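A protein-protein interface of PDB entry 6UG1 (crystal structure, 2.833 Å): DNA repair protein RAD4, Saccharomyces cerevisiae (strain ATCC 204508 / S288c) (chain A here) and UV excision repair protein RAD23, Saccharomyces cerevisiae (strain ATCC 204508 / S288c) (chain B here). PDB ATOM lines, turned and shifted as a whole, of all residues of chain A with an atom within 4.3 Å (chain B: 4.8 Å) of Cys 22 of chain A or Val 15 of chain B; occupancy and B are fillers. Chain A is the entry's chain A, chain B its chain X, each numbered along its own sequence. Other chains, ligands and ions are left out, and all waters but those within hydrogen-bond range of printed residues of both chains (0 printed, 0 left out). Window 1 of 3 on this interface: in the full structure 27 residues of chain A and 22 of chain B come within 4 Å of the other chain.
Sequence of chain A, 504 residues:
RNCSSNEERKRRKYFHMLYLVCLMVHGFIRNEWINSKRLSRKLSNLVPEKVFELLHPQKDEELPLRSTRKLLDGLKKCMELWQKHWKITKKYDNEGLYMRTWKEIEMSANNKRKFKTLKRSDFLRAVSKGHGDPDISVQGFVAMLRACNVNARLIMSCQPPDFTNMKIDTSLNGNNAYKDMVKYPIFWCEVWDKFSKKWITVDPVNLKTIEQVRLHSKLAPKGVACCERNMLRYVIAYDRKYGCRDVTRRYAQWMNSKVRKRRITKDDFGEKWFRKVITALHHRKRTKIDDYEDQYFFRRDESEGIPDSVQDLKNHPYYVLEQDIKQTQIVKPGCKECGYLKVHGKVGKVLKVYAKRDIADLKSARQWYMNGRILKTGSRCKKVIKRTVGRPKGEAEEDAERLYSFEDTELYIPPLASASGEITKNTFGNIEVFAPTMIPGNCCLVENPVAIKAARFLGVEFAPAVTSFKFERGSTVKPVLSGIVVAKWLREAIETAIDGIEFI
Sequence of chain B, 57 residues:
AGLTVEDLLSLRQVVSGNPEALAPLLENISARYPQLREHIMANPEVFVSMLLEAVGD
ND1 of His 26 of chain A is in hydrogen-bond range of O of Val 15 of chain B (2.6 Å).
A ring nitrogen (ND1) of His 26 of chain A lies close to the backbone carbonyl oxygen (O) of Ser 16 of chain B (3.4 Å).
The backbone carbonyl oxygen of Arg 12 of chain B sits at hydrogen-bond distance from the side-chain hydroxyl of Ser 16 of chain B (2.7 Å).
O of Leu 18 of chain A is in hydrogen-bond range of SG of Cys 22 of chain A (3.5 Å).
Leu 26 of chain B touches Leu 18 of chain A.
Val 15 of chain B touches Cys 22 of chain A (CG2 to CB, 3.96 Å).
Leu 22 of chain B touches Cys 22 of chain A.
Cys 22 of chain A touches Leu 26 of chain B.
Val 25 of chain A touches Val 15 of chain B (CG1 to CG1, 3.7 Å).
Pro 19 of chain B touches His 26 of chain A (CG to ND1, 3.3 Å).
Of chain B, only Val 15 (3.96 Å), Leu 22 (3.6 Å) and Leu 26 (3.9 Å) come within 4 Å of Cys 22 of chain A.
Of the printed residues of chain A, Pro 19 of chain B touches His 26.
Of the printed residues of chain A, Leu 26 of chain B touches Leu 18 and Cys 22.
The nearest printed residue of chain B that does not touch Cys 22 of chain A is Leu 11 of chain B (5.2 Å).
Of the 11 printed residues of chain B, 5 touch a printed residue of chain A.
Hydrophobic or aromatic side chains of chain B within 4 Å of the printed part of chain A: Val 15, Pro 19, Leu 22 and Leu 26.
Of the 9 printed residues of chain A, 4 touch a printed residue of chain B.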
ATOM      1  N   LEU A  18     -16.589  -6.295 -35.870  1.00  0.00           N
ATOM      2  CA  LEU A  18     -15.753  -7.045 -34.948  1.00  0.00           C
ATOM      3  C   LEU A  18     -15.593  -6.248 -33.681  1.00  0.00           C
ATOM      4  O   LEU A  18     -15.980  -6.674 -32.580  1.00  0.00           O
ATOM      5  CB  LEU A  18     -14.389  -7.239 -35.590  1.00  0.00           C
ATOM      6  CG  LEU A  18     -13.308  -7.947 -34.770  1.00  0.00           C
ATOM      7  CD1 LEU A  18     -13.875  -9.323 -34.462  1.00  0.00           C
ATOM      8  CD2 LEU A  18     -11.881  -8.028 -35.404  1.00  0.00           C
ATOM      9  N   TYR A  19     -15.261  -4.995 -33.899  1.00  0.00           N
ATOM     10  CA  TYR A  19     -15.020  -4.017 -32.855  1.00  0.00           C
ATOM     11  C   TYR A  19     -16.317  -3.805 -32.066  1.00  0.00           C
ATOM     12  O   TYR A  19     -16.323  -3.713 -30.827  1.00  0.00           O
ATOM     13  CB  TYR A  19     -14.488  -2.810 -33.579  1.00  0.00           C
ATOM     14  CG  TYR A  19     -13.706  -1.938 -32.787  1.00  0.00           C
ATOM     15  CD1 TYR A  19     -14.287  -1.209 -31.773  1.00  0.00           C
ATOM     16  CD2 TYR A  19     -12.306  -1.851 -33.029  1.00  0.00           C
ATOM     17  CE1 TYR A  19     -13.509  -0.347 -30.972  1.00  0.00           C
ATOM     18  CE2 TYR A  19     -11.504  -1.006 -32.256  1.00  0.00           C
ATOM     19  CZ  TYR A  19     -12.136  -0.244 -31.208  1.00  0.00           C
ATOM     20  OH  TYR A  19     -11.465   0.634 -30.387  1.00  0.00           O
ATOM     21  N   LEU A  20     -17.447  -3.774 -32.771  1.00  0.00           N
ATOM     22  CA  LEU A  20     -18.723  -3.619 -32.088  1.00  0.00           C
ATOM     23  C   LEU A  20     -18.923  -4.805 -31.162  1.00  0.00           C
ATOM     24  O   LEU A  20     -19.369  -4.638 -30.020  1.00  0.00           O
ATOM     25  CB  LEU A  20     -19.889  -3.500 -33.084  1.00  0.00           C
ATOM     26  CG  LEU A  20     -21.305  -3.426 -32.528  1.00  0.00           C
ATOM     27  CD1 LEU A  20     -21.533  -2.155 -31.651  1.00  0.00           C
ATOM     28  CD2 LEU A  20     -22.393  -3.505 -33.634  1.00  0.00           C
ATOM     29  N   VAL A  21     -18.728  -6.025 -31.677  1.00  0.00           N
ATOM     30  CA  VAL A  21     -19.001  -7.213 -30.861  1.00  0.00           C
ATOM     31  C   VAL A  21     -18.152  -7.179 -29.599  1.00  0.00           C
ATOM     32  O   VAL A  21     -18.620  -7.414 -28.487  1.00  0.00           O
ATOM     33  CB  VAL A  21     -18.744  -8.494 -31.666  1.00  0.00           C
ATOM     34  CG1 VAL A  21     -18.888  -9.663 -30.780  1.00  0.00           C
ATOM     35  CG2 VAL A  21     -19.702  -8.607 -32.754  1.00  0.00           C
ATOM     36  N   CYS A  22     -16.883  -6.876 -29.764  1.00  0.00           N
ATOM     37  CA  CYS A  22     -16.015  -6.714 -28.609  1.00  0.00           C
ATOM     38  C   CYS A  22     -16.554  -5.693 -27.614  1.00  0.00           C
ATOM     39  O   CYS A  22     -16.808  -6.034 -26.464  1.00  0.00           O
ATOM     40  CB  CYS A  22     -14.614  -6.315 -29.101  1.00  0.00           C
ATOM     41  SG  CYS A  22     -13.730  -7.660 -30.069  1.00  0.00           S
ATOM     42  N   LEU A  23     -16.865  -4.470 -28.078  1.00  0.00           N
ATOM     43  CA  LEU A  23     -17.425  -3.430 -27.204  1.00  0.00           C
ATOM     44  C   LEU A  23     -18.611  -3.972 -26.425  1.00  0.00           C
ATOM     45  O   LEU A  23     -18.676  -3.867 -25.202  1.00  0.00           O
ATOM     46  CB  LEU A  23     -17.831  -2.242 -28.041  1.00  0.00           C
ATOM     47  CG  LEU A  23     -16.659  -1.320 -28.476  1.00  0.00           C
ATOM     48  CD1 LEU A  23     -17.118  -0.191 -29.454  1.00  0.00           C
ATOM     49  CD2 LEU A  23     -15.835  -0.810 -27.330  1.00  0.00           C
ATOM     50  N   MET A  24     -19.593  -4.497 -27.136  1.00  0.00           N
ATOM     51  CA  MET A  24     -20.810  -4.965 -26.484  1.00  0.00           C
ATOM     52  C   MET A  24     -20.542  -6.093 -25.496  1.00  0.00           C
ATOM     53  O   MET A  24     -21.185  -6.155 -24.440  1.00  0.00           O
ATOM     54  CB  MET A  24     -21.815  -5.436 -27.531  1.00  0.00           C
ATOM     55  CG  MET A  24     -22.145  -4.422 -28.534  1.00  0.00           C
ATOM     56  SD  MET A  24     -23.371  -5.084 -29.675  1.00  0.00           S
ATOM     57  CE  MET A  24     -24.985  -5.483 -28.818  1.00  0.00           C
ATOM     58  N   VAL A  25     -19.608  -6.989 -25.810  1.00  0.00           N
ATOM     59  CA  VAL A  25     -19.205  -8.006 -24.818  1.00  0.00           C
ATOM     60  C   VAL A  25     -18.569  -7.356 -23.589  1.00  0.00           C
ATOM     61  O   VAL A  25     -18.762  -7.807 -22.459  1.00  0.00           O
ATOM     62  CB  VAL A  25     -18.228  -9.008 -25.472  1.00  0.00           C
ATOM     63  CG1 VAL A  25     -17.507  -9.928 -24.413  1.00  0.00           C
ATOM     64  CG2 VAL A  25     -18.916  -9.786 -26.667  1.00  0.00           C
ATOM     65  N   HIS A  26     -17.715  -6.358 -23.805  1.00  0.00           N
ATOM     66  CA  HIS A  26     -17.085  -5.676 -22.691  1.00  0.00           C
ATOM     67  C   HIS A  26     -18.151  -5.139 -21.790  1.00  0.00           C
ATOM     68  O   HIS A  26     -17.973  -5.077 -20.574  1.00  0.00           O
ATOM     69  CB  HIS A  26     -16.230  -4.513 -23.179  1.00  0.00           C
ATOM     70  CG  HIS A  26     -15.767  -3.613 -22.080  1.00  0.00           C
ATOM     71  ND1 HIS A  26     -14.585  -3.781 -21.410  1.00  0.00           N
ATOM     72  CD2 HIS A  26     -16.338  -2.497 -21.557  1.00  0.00           C
ATOM     73  CE1 HIS A  26     -14.458  -2.843 -20.493  1.00  0.00           C
ATOM     74  NE2 HIS A  26     -15.495  -2.029 -20.584  1.00  0.00           N
ATOM     75  N   LEU B  11      -7.578 -12.277 -25.219  1.00  0.00           N
ATOM     76  CA  LEU B  11      -8.542 -11.421 -25.864  1.00  0.00           C
ATOM     77  C   LEU B  11      -9.696 -11.139 -24.902  1.00  0.00           C
ATOM     78  O   LEU B  11     -10.097  -9.979 -24.720  1.00  0.00           O
ATOM     79  CB  LEU B  11      -9.165 -12.129 -27.067  1.00  0.00           C
ATOM     80  CG  LEU B  11     -10.056 -11.217 -27.949  1.00  0.00           C
ATOM     81  CD1 LEU B  11      -9.147 -10.097 -28.494  1.00  0.00           C
ATOM     82  CD2 LEU B  11     -10.896 -11.822 -28.984  1.00  0.00           C
ATOM     83  N   ARG B  12     -10.153 -12.175 -24.189  1.00  0.00           N
ATOM     84  CA  ARG B  12     -11.101 -11.959 -23.108  1.00  0.00           C
ATOM     85  C   ARG B  12     -10.532 -10.962 -22.119  1.00  0.00           C
ATOM     86  O   ARG B  12     -11.270 -10.182 -21.515  1.00  0.00           O
ATOM     87  CB  ARG B  12     -11.513 -13.248 -22.410  1.00  0.00           C
ATOM     88  CG  ARG B  12     -12.276 -12.967 -21.085  1.00  0.00           C
ATOM     89  CD  ARG B  12     -12.909 -14.174 -20.466  1.00  0.00           C
ATOM     90  NE  ARG B  12     -13.721 -13.853 -19.275  1.00  0.00           N
ATOM     91  CZ  ARG B  12     -15.023 -14.048 -19.119  1.00  0.00           C
ATOM     92  NH1 ARG B  12     -15.735 -14.595 -20.068  1.00  0.00           N
ATOM     93  NH2 ARG B  12     -15.613 -13.743 -17.977  1.00  0.00           N
ATOM     94  N   GLN B  13      -9.235 -10.995 -21.880  1.00  0.00           N
ATOM     95  CA  GLN B  13      -8.733 -10.130 -20.819  1.00  0.00           C
ATOM     96  C   GLN B  13      -8.703  -8.674 -21.286  1.00  0.00           C
ATOM     97  O   GLN B  13      -9.051  -7.774 -20.516  1.00  0.00           O
ATOM     98  CB  GLN B  13      -7.340 -10.590 -20.373  1.00  0.00           C
ATOM     99  CG  GLN B  13      -7.309 -12.049 -19.923  1.00  0.00           C
ATOM    100  CD  GLN B  13      -5.947 -12.573 -19.576  1.00  0.00           C
ATOM    101  OE1 GLN B  13      -5.870 -13.600 -18.914  1.00  0.00           O
ATOM    102  NE2 GLN B  13      -4.866 -11.896 -20.013  1.00  0.00           N
ATOM    103  N   VAL B  14      -8.238  -8.417 -22.500  1.00  0.00           N
ATOM    104  CA  VAL B  14      -8.291  -7.060 -23.056  1.00  0.00           C
ATOM    105  C   VAL B  14      -9.739  -6.569 -23.125  1.00  0.00           C
ATOM    106  O   VAL B  14     -10.062  -5.407 -22.827  1.00  0.00           O
ATOM    107  CB  VAL B  14      -7.640  -6.965 -24.423  1.00  0.00           C
ATOM    108  CG1 VAL B  14      -8.037  -5.685 -24.988  1.00  0.00           C
ATOM    109  CG2 VAL B  14      -6.157  -7.056 -24.289  1.00  0.00           C
ATOM    110  N   VAL B  15     -10.588  -7.376 -23.743  1.00  0.00           N
ATOM    111  CA  VAL B  15     -11.998  -7.013 -23.883  1.00  0.00           C
ATOM    112  C   VAL B  15     -12.589  -6.685 -22.526  1.00  0.00           C
ATOM    113  O   VAL B  15     -13.477  -5.866 -22.421  1.00  0.00           O
ATOM    114  CB  VAL B  15     -12.801  -8.122 -24.603  1.00  0.00           C
ATOM    115  CG1 VAL B  15     -14.304  -8.160 -24.205  1.00  0.00           C
ATOM    116  CG2 VAL B  15     -12.672  -8.002 -26.091  1.00  0.00           C
ATOM    117  N   SER B  16     -12.196  -7.378 -21.494  1.00  0.00           N
ATOM    118  CA  SER B  16     -12.797  -7.150 -20.186  1.00  0.00           C
ATOM    119  C   SER B  16     -12.257  -5.910 -19.471  1.00  0.00           C
ATOM    120  O   SER B  16     -13.007  -5.252 -18.722  1.00  0.00           O
ATOM    121  CB  SER B  16     -12.580  -8.361 -19.307  1.00  0.00           C
ATOM    122  OG  SER B  16     -13.234  -9.475 -19.858  1.00  0.00           O
ATOM    123  N   GLY B  17     -10.935  -5.764 -19.417  1.00  0.00           N
ATOM    124  CA  GLY B  17     -10.412  -4.654 -18.638  1.00  0.00           C
ATOM    125  C   GLY B  17      -9.658  -3.558 -19.335  1.00  0.00           C
ATOM    126  O   GLY B  17      -9.527  -2.481 -18.756  1.00  0.00           O
ATOM    127  N   PRO B  19     -10.258  -2.291 -22.980  1.00  0.00           N
ATOM    128  CA  PRO B  19     -10.705  -2.310 -24.393  1.00  0.00           C
ATOM    129  C   PRO B  19     -10.157  -1.171 -25.224  1.00  0.00           C
ATOM    130  O   PRO B  19     -10.120  -1.291 -26.451  1.00  0.00           O
ATOM    131  CB  PRO B  19     -12.230  -2.305 -24.297  1.00  0.00           C
ATOM    132  CG  PRO B  19     -12.533  -1.774 -22.965  1.00  0.00           C
ATOM    133  CD  PRO B  19     -11.389  -2.142 -22.051  1.00  0.00           C
ATOM    134  N   LEU B  22      -7.712  -2.786 -27.537  1.00  0.00           N
ATOM    135  CA  LEU B  22      -8.185  -3.784 -28.512  1.00  0.00           C
ATOM    136  C   LEU B  22      -7.513  -3.714 -29.882  1.00  0.00           C
ATOM    137  O   LEU B  22      -7.041  -4.723 -30.396  1.00  0.00           O
ATOM    138  CB  LEU B  22      -9.700  -3.635 -28.645  1.00  0.00           C
ATOM    139  CG  LEU B  22     -10.417  -4.615 -27.726  1.00  0.00           C
ATOM    140  CD1 LEU B  22     -11.914  -4.436 -27.692  1.00  0.00           C
ATOM    141  CD2 LEU B  22     -10.197  -5.970 -28.294  1.00  0.00           C
ATOM    142  N   LEU B  26      -6.483  -7.200 -32.240  1.00  0.00           N
ATOM    143  CA  LEU B  26      -7.436  -7.675 -33.250  1.00  0.00           C
ATOM    144  C   LEU B  26      -6.822  -7.666 -34.626  1.00  0.00           C
ATOM    145  O   LEU B  26      -7.137  -8.527 -35.461  1.00  0.00           O
ATOM    146  CB  LEU B  26      -8.669  -6.785 -33.327  1.00  0.00           C
ATOM    147  CG  LEU B  26      -9.686  -6.664 -32.214  1.00  0.00           C
ATOM    148  CD1 LEU B  26     -10.757  -5.723 -32.718  1.00  0.00           C
ATOM    149  CD2 LEU B  26     -10.268  -8.039 -31.902  1.00  0.00           C
ATOM    150  N   LEU B  51     -16.062 -16.075 -25.749  1.00  0.00           N
ATOM    151  CA  LEU B  51     -15.497 -14.982 -24.930  1.00  0.00           C
ATOM    152  C   LEU B  51     -16.110 -14.825 -23.530  1.00  0.00           C
ATOM    153  O   LEU B  51     -15.472 -14.243 -22.649  1.00  0.00           O
ATOM    154  CB  LEU B  51     -15.677 -13.694 -25.682  1.00  0.00           C
ATOM    155  CG  LEU B  51     -14.450 -13.478 -26.559  1.00  0.00           C
ATOM    156  CD1 LEU B  51     -14.728 -14.183 -27.856  1.00  0.00           C
ATOM    157  CD2 LEU B  51     -14.091 -12.076 -26.838  1.00  0.00           C
